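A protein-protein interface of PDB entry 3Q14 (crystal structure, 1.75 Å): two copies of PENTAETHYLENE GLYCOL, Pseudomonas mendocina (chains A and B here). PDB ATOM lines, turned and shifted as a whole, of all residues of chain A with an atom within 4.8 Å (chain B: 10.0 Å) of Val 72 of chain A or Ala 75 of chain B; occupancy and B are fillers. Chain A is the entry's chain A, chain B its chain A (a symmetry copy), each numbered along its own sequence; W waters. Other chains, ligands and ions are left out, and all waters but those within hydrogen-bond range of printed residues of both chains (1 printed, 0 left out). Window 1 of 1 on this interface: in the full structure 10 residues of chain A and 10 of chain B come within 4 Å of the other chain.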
ATOM      1  N   GLY A  68      27.389 -10.778  10.713  1.00  0.00           N
ATOM      2  CA  GLY A  68      27.125  -9.380  10.419  1.00  0.00           C
ATOM      3  C   GLY A  68      25.730  -8.928  10.839  1.00  0.00           C
ATOM      4  O   GLY A  68      25.585  -7.906  11.506  1.00  0.00           O
ATOM      5  N   ALA A  69      24.705  -9.682  10.466  1.00  0.00           N
ATOM      6  CA  ALA A  69      23.332  -9.284  10.765  1.00  0.00           C
ATOM      7  C   ALA A  69      23.112  -9.137  12.267  1.00  0.00           C
ATOM      8  O   ALA A  69      22.533  -8.148  12.728  1.00  0.00           O
ATOM      9  CB  ALA A  69      22.338 -10.291  10.198  1.00  0.00           C
ATOM     10  N   TYR A  70      23.557 -10.135  13.026  1.00  0.00           N
ATOM     11  CA  TYR A  70      23.361 -10.119  14.478  1.00  0.00           C
ATOM     12  C   TYR A  70      24.231  -9.086  15.179  1.00  0.00           C
ATOM     13  O   TYR A  70      23.796  -8.480  16.159  1.00  0.00           O
ATOM     14  CB  TYR A  70      23.566 -11.521  15.090  1.00  0.00           C
ATOM     15  CG  TYR A  70      22.475 -12.519  14.694  1.00  0.00           C
ATOM     16  CD1 TYR A  70      21.228 -12.502  15.303  1.00  0.00           C
ATOM     17  CD2 TYR A  70      22.700 -13.473  13.706  1.00  0.00           C
ATOM     18  CE1 TYR A  70      20.237 -13.411  14.937  1.00  0.00           C
ATOM     19  CE2 TYR A  70      21.714 -14.383  13.336  1.00  0.00           C
ATOM     20  CZ  TYR A  70      20.487 -14.349  13.961  1.00  0.00           C
ATOM     21  OH  TYR A  70      19.508 -15.256  13.597  1.00  0.00           O
ATOM     22  N   SER A  71      25.455  -8.880  14.682  1.00  0.00           N
ATOM     23  CA  SER A  71      26.364  -7.919  15.293  1.00  0.00           C
ATOM     24  C   SER A  71      25.812  -6.506  15.180  1.00  0.00           C
ATOM     25  O   SER A  71      25.909  -5.709  16.119  1.00  0.00           O
ATOM     26  CB  SER A  71      27.753  -7.974  14.626  1.00  0.00           C
ATOM     27  OG  SER A  71      28.501  -9.079  15.100  1.00  0.00           O
ATOM     28  N   VAL A  72      25.267  -6.188  14.012  1.00  0.00           N
ATOM     29  CA  VAL A  72      24.683  -4.874  13.809  1.00  0.00           C
ATOM     30  C   VAL A  72      23.478  -4.685  14.731  1.00  0.00           C
ATOM     31  O   VAL A  72      23.356  -3.664  15.411  1.00  0.00           O
ATOM     32  CB  VAL A  72      24.298  -4.646  12.327  1.00  0.00           C
ATOM     33  CG1 VAL A  72      23.527  -3.357  12.180  1.00  0.00           C
ATOM     34  CG2 VAL A  72      25.564  -4.606  11.479  1.00  0.00           C
ATOM     35  N   LYS A  73      22.606  -5.683  14.788  1.00  0.00           N
ATOM     36  CA  LYS A  73      21.441  -5.606  15.670  1.00  0.00           C
ATOM     37  C   LYS A  73      21.879  -5.338  17.109  1.00  0.00           C
ATOM     38  O   LYS A  73      21.345  -4.460  17.787  1.00  0.00           O
ATOM     39  CB  LYS A  73      20.633  -6.906  15.610  1.00  0.00           C
ATOM     40  CG  LYS A  73      19.446  -6.944  16.582  1.00  0.00           C
ATOM     41  CD  LYS A  73      18.764  -8.316  16.577  1.00  0.00           C
ATOM     42  CE  LYS A  73      17.545  -8.365  17.505  1.00  0.00           C
ATOM     43  NZ  LYS A  73      17.907  -8.283  18.955  1.00  0.00           N
ATOM     44  N   ALA A  74      22.857  -6.106  17.569  1.00  0.00           N
ATOM     45  CA  ALA A  74      23.347  -5.963  18.937  1.00  0.00           C
ATOM     46  C   ALA A  74      23.907  -4.566  19.162  1.00  0.00           C
ATOM     47  O   ALA A  74      23.659  -3.953  20.196  1.00  0.00           O
ATOM     48  CB  ALA A  74      24.404  -7.018  19.245  1.00  0.00           C
ATOM     49  N   ALA A  75      24.654  -4.050  18.189  1.00  0.00           N
ATOM     50  CA  ALA A  75      25.328  -2.776  18.397  1.00  0.00           C
ATOM     51  C   ALA A  75      24.364  -1.593  18.413  1.00  0.00           C
ATOM     52  O   ALA A  75      24.701  -0.523  18.928  1.00  0.00           O
ATOM     53  CB  ALA A  75      26.413  -2.566  17.354  1.00  0.00           C
ATOM     54  N   LEU A  76      23.163  -1.790  17.872  1.00  0.00           N
ATOM     55  CA  LEU A  76      22.212  -0.691  17.737  1.00  0.00           C
ATOM     56  C   LEU A  76      20.981  -0.801  18.639  1.00  0.00           C
ATOM     57  O   LEU A  76      20.039  -0.026  18.496  1.00  0.00           O
ATOM     58  CB  LEU A  76      21.773  -0.532  16.285  1.00  0.00           C
ATOM     59  CG  LEU A  76      22.872  -0.202  15.276  1.00  0.00           C
ATOM     60  CD1 LEU A  76      22.267  -0.152  13.874  1.00  0.00           C
ATOM     61  CD2 LEU A  76      23.555   1.114  15.627  1.00  0.00           C
ATOM     62  N   TYR A 218      19.146   1.194  10.557  1.00  0.00           N
ATOM     63  CA  TYR A 218      20.157   0.367   9.915  1.00  0.00           C
ATOM     64  C   TYR A 218      20.091  -1.094  10.321  1.00  0.00           C
ATOM     65  O   TYR A 218      20.475  -1.962   9.548  1.00  0.00           O
ATOM     66  CB  TYR A 218      21.556   0.958  10.091  1.00  0.00           C
ATOM     67  CG  TYR A 218      21.600   2.340   9.517  1.00  0.00           C
ATOM     68  CD1 TYR A 218      21.647   2.534   8.143  1.00  0.00           C
ATOM     69  CD2 TYR A 218      21.546   3.454  10.341  1.00  0.00           C
ATOM     70  CE1 TYR A 218      21.656   3.804   7.604  1.00  0.00           C
ATOM     71  CE2 TYR A 218      21.557   4.734   9.807  1.00  0.00           C
ATOM     72  CZ  TYR A 218      21.612   4.897   8.437  1.00  0.00           C
ATOM     73  OH  TYR A 218      21.620   6.156   7.889  1.00  0.00           O
ATOM     74  N   THR A 219      19.573  -1.377  11.512  1.00  0.00           N
ATOM     75  CA  THR A 219      19.365  -2.767  11.884  1.00  0.00           C
ATOM     76  C   THR A 219      18.476  -3.436  10.859  1.00  0.00           C
ATOM     77  O   THR A 219      18.770  -4.534  10.379  1.00  0.00           O
ATOM     78  CB  THR A 219      18.717  -2.882  13.269  1.00  0.00           C
ATOM     79  OG1 THR A 219      19.660  -2.411  14.235  1.00  0.00           O
ATOM     80  CG2 THR A 219      18.364  -4.333  13.573  1.00  0.00           C
ATOM     81  N   ASN A 222      19.985  -3.324   7.082  1.00  0.00           N
ATOM     82  CA  ASN A 222      21.063  -4.297   7.006  1.00  0.00           C
ATOM     83  C   ASN A 222      20.524  -5.729   6.978  1.00  0.00           C
ATOM     84  O   ASN A 222      21.028  -6.581   6.241  1.00  0.00           O
ATOM     85  CB  ASN A 222      22.025  -4.106   8.179  1.00  0.00           C
ATOM     86  CG  ASN A 222      23.281  -4.942   8.030  1.00  0.00           C
ATOM     87  OD1 ASN A 222      24.096  -4.695   7.138  1.00  0.00           O
ATOM     88  ND2 ASN A 222      23.440  -5.932   8.894  1.00  0.00           N
ATOM     89  N   GLU B  64      36.111 -13.195  16.595  1.00  0.00           N
ATOM     90  CA  GLU B  64      34.747 -12.738  16.779  1.00  0.00           C
ATOM     91  C   GLU B  64      34.664 -11.244  17.116  1.00  0.00           C
ATOM     92  O   GLU B  64      33.800 -10.535  16.590  1.00  0.00           O
ATOM     93  CB  GLU B  64      34.029 -13.592  17.816  1.00  0.00           C
ATOM     94  CG  GLU B  64      32.581 -13.190  18.018  1.00  0.00           C
ATOM     95  CD  GLU B  64      31.786 -14.265  18.728  1.00  0.00           C
ATOM     96  OE1 GLU B  64      30.600 -14.027  19.039  1.00  0.00           O
ATOM     97  OE2 GLU B  64      32.351 -15.355  18.962  1.00  0.00           O
ATOM     98  N   ALA B  67      35.186  -9.250  13.870  1.00  0.00           N
ATOM     99  CA  ALA B  67      34.074  -9.390  12.934  1.00  0.00           C
ATOM    100  C   ALA B  67      32.968  -8.402  13.303  1.00  0.00           C
ATOM    101  O   ALA B  67      32.414  -7.728  12.434  1.00  0.00           O
ATOM    102  CB  ALA B  67      33.543 -10.818  12.925  1.00  0.00           C
ATOM    103  N   GLY B  68      32.672  -8.299  14.598  1.00  0.00           N
ATOM    104  CA  GLY B  68      31.694  -7.338  15.077  1.00  0.00           C
ATOM    105  C   GLY B  68      32.088  -5.890  14.806  1.00  0.00           C
ATOM    106  O   GLY B  68      31.289  -5.119  14.280  1.00  0.00           O
ATOM    107  N   ALA B  69      33.313  -5.515  15.149  1.00  0.00           N
ATOM    108  CA  ALA B  69      33.746  -4.130  14.990  1.00  0.00           C
ATOM    109  C   ALA B  69      33.654  -3.684  13.534  1.00  0.00           C
ATOM    110  O   ALA B  69      33.141  -2.600  13.236  1.00  0.00           O
ATOM    111  CB  ALA B  69      35.173  -3.945  15.493  1.00  0.00           C
ATOM    112  N   TYR B  70      34.172  -4.513  12.633  1.00  0.00           N
ATOM    113  CA  TYR B  70      34.176  -4.165  11.209  1.00  0.00           C
ATOM    114  C   TYR B  70      32.790  -4.218  10.585  1.00  0.00           C
ATOM    115  O   TYR B  70      32.476  -3.403   9.717  1.00  0.00           O
ATOM    116  CB  TYR B  70      35.172  -5.042  10.418  1.00  0.00           C
ATOM    117  CG  TYR B  70      36.635  -4.752  10.759  1.00  0.00           C
ATOM    118  CD1 TYR B  70      37.290  -3.644  10.238  1.00  0.00           C
ATOM    119  CD2 TYR B  70      37.354  -5.589  11.607  1.00  0.00           C
ATOM    120  CE1 TYR B  70      38.622  -3.383  10.553  1.00  0.00           C
ATOM    121  CE2 TYR B  70      38.684  -5.333  11.925  1.00  0.00           C
ATOM    122  CZ  TYR B  70      39.313  -4.231  11.389  1.00  0.00           C
ATOM    123  OH  TYR B  70      40.636  -3.978  11.702  1.00  0.00           O
ATOM    124  N   SER B  71      31.957  -5.168  11.023  1.00  0.00           N
ATOM    125  CA  SER B  71      30.614  -5.303  10.478  1.00  0.00           C
ATOM    126  C   SER B  71      29.774  -4.075  10.797  1.00  0.00           C
ATOM    127  O   SER B  71      29.005  -3.595   9.959  1.00  0.00           O
ATOM    128  CB  SER B  71      29.913  -6.555  11.042  1.00  0.00           C
ATOM    129  OG  SER B  71      30.365  -7.728  10.389  1.00  0.00           O
ATOM    130  N   VAL B  72      29.897  -3.593  12.028  1.00  0.00           N
ATOM    131  CA  VAL B  72      29.164  -2.405  12.427  1.00  0.00           C
ATOM    132  C   VAL B  72      29.634  -1.198  11.614  1.00  0.00           C
ATOM    133  O   VAL B  72      28.821  -0.445  11.073  1.00  0.00           O
ATOM    134  CB  VAL B  72      29.290  -2.143  13.947  1.00  0.00           C
ATOM    135  CG1 VAL B  72      28.680  -0.809  14.300  1.00  0.00           C
ATOM    136  CG2 VAL B  72      28.593  -3.263  14.711  1.00  0.00           C
ATOM    137  N   LYS B  73      30.944  -1.033  11.492  1.00  0.00           N
ATOM    138  CA  LYS B  73      31.485   0.074  10.703  1.00  0.00           C
ATOM    139  C   LYS B  73      30.924   0.040   9.282  1.00  0.00           C
ATOM    140  O   LYS B  73      30.463   1.052   8.753  1.00  0.00           O
ATOM    141  CB  LYS B  73      33.015   0.004  10.655  1.00  0.00           C
ATOM    142  CG  LYS B  73      33.658   1.077   9.765  1.00  0.00           C
ATOM    143  CD  LYS B  73      35.171   0.869   9.646  1.00  0.00           C
ATOM    144  CE  LYS B  73      35.843   1.956   8.799  1.00  0.00           C
ATOM    145  NZ  LYS B  73      35.477   1.882   7.350  1.00  0.00           N
ATOM    146  N   ALA B  74      30.969  -1.135   8.670  1.00  0.00           N
ATOM    147  CA  ALA B  74      30.486  -1.290   7.301  1.00  0.00           C
ATOM    148  C   ALA B  74      29.007  -0.943   7.213  1.00  0.00           C
ATOM    149  O   ALA B  74      28.578  -0.271   6.279  1.00  0.00           O
ATOM    150  CB  ALA B  74      30.732  -2.708   6.799  1.00  0.00           C
ATOM    151  N   ALA B  75      28.222  -1.387   8.191  1.00  0.00           N
ATOM    152  CA  ALA B  75      26.781  -1.204   8.098  1.00  0.00           C
ATOM    153  C   ALA B  75      26.356   0.250   8.288  1.00  0.00           C
ATOM    154  O   ALA B  75      25.254   0.633   7.887  1.00  0.00           O
ATOM    155  CB  ALA B  75      26.060  -2.104   9.086  1.00  0.00           C
ATOM    156  N   LEU B  76      27.234   1.060   8.878  1.00  0.00           N
ATOM    157  CA  LEU B  76      26.880   2.437   9.206  1.00  0.00           C
ATOM    158  C   LEU B  76      27.612   3.497   8.379  1.00  0.00           C
ATOM    159  O   LEU B  76      27.520   4.685   8.676  1.00  0.00           O
ATOM    160  CB  LEU B  76      27.093   2.709  10.692  1.00  0.00           C
ATOM    161  CG  LEU B  76      26.263   1.867  11.661  1.00  0.00           C
ATOM    162  CD1 LEU B  76      26.656   2.221  13.095  1.00  0.00           C
ATOM    163  CD2 LEU B  76      24.773   2.085  11.431  1.00  0.00           C
ATOM    164  N   GLU B  77      28.317   3.077   7.339  1.00  0.00           N
ATOM    165  CA  GLU B  77      29.065   4.029   6.523  1.00  0.00           C
ATOM    166  C   GLU B  77      28.206   5.193   6.028  1.00  0.00           C
ATOM    167  O   GLU B  77      28.713   6.298   5.829  1.00  0.00           O
ATOM    168  CB  GLU B  77      29.688   3.328   5.314  1.00  0.00           C
ATOM    169  CG  GLU B  77      30.687   2.246   5.663  1.00  0.00           C
ATOM    170  CD  GLU B  77      31.976   2.807   6.236  1.00  0.00           C
ATOM    171  OE1 GLU B  77      32.916   2.019   6.474  1.00  0.00           O
ATOM    172  OE2 GLU B  77      32.050   4.036   6.452  1.00  0.00           O
ATOM    173  N   ARG B  78      26.919   4.944   5.814  1.00  0.00           N
ATOM    174  CA  ARG B  78      26.051   5.931   5.181  1.00  0.00           C
ATOM    175  C   ARG B  78      25.148   6.636   6.187  1.00  0.00           C
ATOM    176  O   ARG B  78      24.175   7.293   5.801  1.00  0.00           O
ATOM    177  CB  ARG B  78      25.187   5.279   4.097  1.00  0.00           C
ATOM    178  CG  ARG B  78      25.950   4.521   3.016  1.00  0.00           C
ATOM    179  CD  ARG B  78      26.914   5.423   2.238  1.00  0.00           C
ATOM    180  NE  ARG B  78      26.253   6.590   1.658  1.00  0.00           N
ATOM    181  CZ  ARG B  78      25.561   6.578   0.524  1.00  0.00           C
ATOM    182  NH1 ARG B  78      25.420   5.450  -0.167  1.00  0.00           N
ATOM    183  NH2 ARG B  78      25.001   7.697   0.081  1.00  0.00           N
ATOM    184  N   ALA B  79      25.472   6.510   7.469  1.00  0.00           N
ATOM    185  CA  ALA B  79      24.667   7.118   8.526  1.00  0.00           C
ATOM    186  C   ALA B  79      24.872   8.638   8.652  1.00  0.00           C
ATOM    187  O   ALA B  79      24.259   9.287   9.500  1.00  0.00           O
ATOM    188  CB  ALA B  79      24.927   6.426   9.859  1.00  0.00           C
ATOM    189  N   LYS B  80      25.732   9.196   7.805  1.00  0.00           N
ATOM    190  CA  LYS B  80      25.923  10.643   7.736  1.00  0.00           C
ATOM    191  C   LYS B  80      26.549  11.228   9.000  1.00  0.00           C
ATOM    192  O   LYS B  80      26.335  12.402   9.307  1.00  0.00           O
ATOM    193  CB  LYS B  80      24.589  11.355   7.478  1.00  0.00           C
ATOM    194  CG  LYS B  80      23.683  10.676   6.462  1.00  0.00           C
ATOM    195  CD  LYS B  80      23.460  11.554   5.238  1.00  0.00           C
ATOM    196  CE  LYS B  80      24.748  11.743   4.450  1.00  0.00           C
ATOM    197  NZ  LYS B  80      24.517  12.490   3.181  1.00  0.00           N
ATOM    198  N   ILE B  81      27.312  10.422   9.737  1.00  0.00           N
ATOM    199  CA  ILE B  81      27.965  10.921  10.945  1.00  0.00           C
ATOM    200  C   ILE B  81      28.832  12.139  10.654  1.00  0.00           C
ATOM    201  O   ILE B  81      28.704  13.177  11.308  1.00  0.00           O
ATOM    202  CB  ILE B  81      28.821   9.835  11.631  1.00  0.00           C
ATOM    203  CG1 ILE B  81      27.914   8.787  12.270  1.00  0.00           C
ATOM    204  CG2 ILE B  81      29.730  10.459  12.697  1.00  0.00           C
ATOM    205  CD1 ILE B  81      27.023   9.340  13.351  1.00  0.00           C
ATOM    206  N   PHE B 144      39.956   2.780  10.952  1.00  0.00           N
ATOM    207  CA  PHE B 144      38.680   3.474  11.107  1.00  0.00           C
ATOM    208  C   PHE B 144      38.715   4.918  10.618  1.00  0.00           C
ATOM    209  O   PHE B 144      37.844   5.330   9.848  1.00  0.00           O
ATOM    210  CB  PHE B 144      38.133   3.351  12.542  1.00  0.00           C
ATOM    211  CG  PHE B 144      37.343   2.083  12.775  1.00  0.00           C
ATOM    212  CD1 PHE B 144      37.906   0.838  12.525  1.00  0.00           C
ATOM    213  CD2 PHE B 144      36.034   2.138  13.232  1.00  0.00           C
ATOM    214  CE1 PHE B 144      37.180  -0.338  12.731  1.00  0.00           C
ATOM    215  CE2 PHE B 144      35.298   0.968  13.448  1.00  0.00           C
ATOM    216  CZ  PHE B 144      35.870  -0.274  13.193  1.00  0.00           C
ATOM    217  N   GLU B 147      39.144   6.219   6.313  1.00  0.00           N
ATOM    218  CA  GLU B 147      38.148   6.562   5.307  1.00  0.00           C
ATOM    219  C   GLU B 147      37.818   8.052   5.287  1.00  0.00           C
ATOM    220  O   GLU B 147      37.284   8.551   4.303  1.00  0.00           O
ATOM    221  CB  GLU B 147      36.873   5.736   5.464  1.00  0.00           C
ATOM    222  CG  GLU B 147      36.097   6.019   6.721  1.00  0.00           C
ATOM    223  CD  GLU B 147      34.657   5.565   6.597  1.00  0.00           C
ATOM    224  OE1 GLU B 147      34.162   4.896   7.524  1.00  0.00           O
ATOM    225  OE2 GLU B 147      34.024   5.879   5.567  1.00  0.00           O
ATOM    226  N   TYR B 218      27.537   5.128  16.745  1.00  0.00           N
ATOM    227  CA  TYR B 218      27.682   3.759  17.215  1.00  0.00           C
ATOM    228  C   TYR B 218      28.893   3.047  16.639  1.00  0.00           C
ATOM    229  O   TYR B 218      29.437   2.153  17.274  1.00  0.00           O
ATOM    230  CB  TYR B 218      26.392   2.962  17.023  1.00  0.00           C
ATOM    231  CG  TYR B 218      25.269   3.627  17.757  1.00  0.00           C
ATOM    232  CD1 TYR B 218      25.173   3.529  19.139  1.00  0.00           C
ATOM    233  CD2 TYR B 218      24.333   4.393  17.081  1.00  0.00           C
ATOM    234  CE1 TYR B 218      24.159   4.165  19.828  1.00  0.00           C
ATOM    235  CE2 TYR B 218      23.310   5.034  17.765  1.00  0.00           C
ATOM    236  CZ  TYR B 218      23.234   4.912  19.139  1.00  0.00           C
ATOM    237  OH  TYR B 218      22.231   5.542  19.835  1.00  0.00           O
ATOM    238  N   THR B 219      29.343   3.459  15.458  1.00  0.00           N
ATOM    239  CA  THR B 219      30.578   2.900  14.933  1.00  0.00           C
ATOM    240  C   THR B 219      31.698   3.131  15.924  1.00  0.00           C
ATOM    241  O   THR B 219      32.463   2.219  16.246  1.00  0.00           O
ATOM    242  CB  THR B 219      30.950   3.537  13.589  1.00  0.00           C
ATOM    243  OG1 THR B 219      29.966   3.144  12.630  1.00  0.00           O
ATOM    244  CG2 THR B 219      32.322   3.054  13.134  1.00  0.00           C
ATOM    245  N   ASN B 222      30.991   1.494  19.581  1.00  0.00           N
ATOM    246  CA  ASN B 222      31.183   0.057  19.468  1.00  0.00           C
ATOM    247  C   ASN B 222      32.666  -0.304  19.355  1.00  0.00           C
ATOM    248  O   ASN B 222      33.127  -1.282  19.949  1.00  0.00           O
ATOM    249  CB  ASN B 222      30.405  -0.483  18.268  1.00  0.00           C
ATOM    250  CG  ASN B 222      30.388  -1.998  18.232  1.00  0.00           C
ATOM    251  OD1 ASN B 222      29.780  -2.639  19.094  1.00  0.00           O
ATOM    252  ND2 ASN B 222      31.054  -2.576  17.246  1.00  0.00           N
HETATM  253  O   HOH W   1      30.245  -9.945  12.624  1.00  0.00           O
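The side-chain hydroxyl (OH) of Tyr 218 of chain A is in hydrogen-bond range of the backbone carbonyl oxygen (O) of Arg 78 of chain B (3.5 Å).
O of Ala 67 of chain B is in hydrogen-bond range of OG of Ser 71 of chain B (2.9 Å).
Among the printed residues, pairs that only touch across the chains: Tyr 218 of chain A with Ala 79 of chain B, Ala 75 of chain A with Val 72 of chain B, Val 72 of chain A with Ala 75 of chain B, Ser 71 of chain A with Gly 68 of chain B, Gly 68 of chain A with Ser 71 of chain B, Leu 76 of chain A with Tyr 218 of chain B, Tyr 218 of chain A with Leu 76 of chain B, Asn 222 of chain A with Ala 75 of chain B, Ala 75 of chain A with Asn 222 of chain B, Ser 71 of chain A with Val 72 of chain B and Val 72 of chain A with Ser 71 of chain B.
Of chain A, only Val 72 and Asn 222 come within 4 Å of Ala 75 of chain B.
Of chain B, only Gly 68 and Val 72 come within 4 Å of Ser 71 of chain A.
Ala 75 of chain A touches just these residues of chain B: Val 72 (3.5 Å) and Asn 222 (3.8 Å).
No residue of chain B comes within 4 Å of Thr 219 of chain A.
Of the printed residues of chain B, Tyr 218 of chain A touches Leu 76, Arg 78 and Ala 79.
Of the printed residues of chain A, Ala 79 of chain B touches Tyr 218.
Of the printed residues of chain A, Asn 222 of chain B touches Ala 75.
Printed residues of chain A within 4 Å of Ser 71 of chain B: Gly 68 (3.6 Å) and Val 72 (3.9 Å).
Of the printed residues of chain A, Val 72 of chain B touches Ser 71 (3.9 Å) and Ala 75 (3.5 Å).
Ala 67 of chain B touches none of the printed residues of chain A.
Ala 69 of chain B touches none of the printed residues of chain A.
The nearest residue of chain B that does not touch Val 72 of chain A is Val 72 of chain B (4.3 Å).
Of the 12 printed residues of chain A, 7 touch a printed residue of chain B.
Hydrophobic or aromatic side chains of chain A within 4 Å of the printed part of chain B: Val 72, Ala 75, Leu 76 and Tyr 218.
Hydrophobic or aromatic side chains of chain B that line the printed part of chain A: Val 72, Ala 75, Leu 76, Ala 79 and Tyr 218.
Among the printed residues, 12 pairs touch across the chains.
Among the printed residues, no Asp or Glu carboxylate lies within 4 Å of a Lys or Arg side-chain nitrogen of the other chain.
Ser 71 of chain A touches Val 72 of chain B, and with the chains exchanged Val 72 of chain A touches Ser 71 of chain B.
Val 72 of chain A touches Ala 75 of chain B, and with the chains exchanged Ala 75 of chain A touches Val 72 of chain B.
Ala 75 of chain A touches Asn 222 of chain B, and with the chains exchanged Asn 222 of chain A touches Ala 75 of chain B.
Leu 76 of chain A touches Tyr 218 of chain B, and with the chains exchanged Tyr 218 of chain A touches Leu 76 of chain B.
Positions printed for both chains: 68, 69, 70, 71, 72, 73, 74, 75, 76, 218, 219 and 222.
Of the 12 pairs that touch across the chains among the printed residues, 10 have their exchanged pair printed and touching as well.
Water W1 lies within hydrogen-bond range of the backbone carbonyl oxygen of Ala 67 of chain B, the side-chain hydroxyl of Ser 71 of chain A and the side-chain hydroxyl of Ser 71 of chain B.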
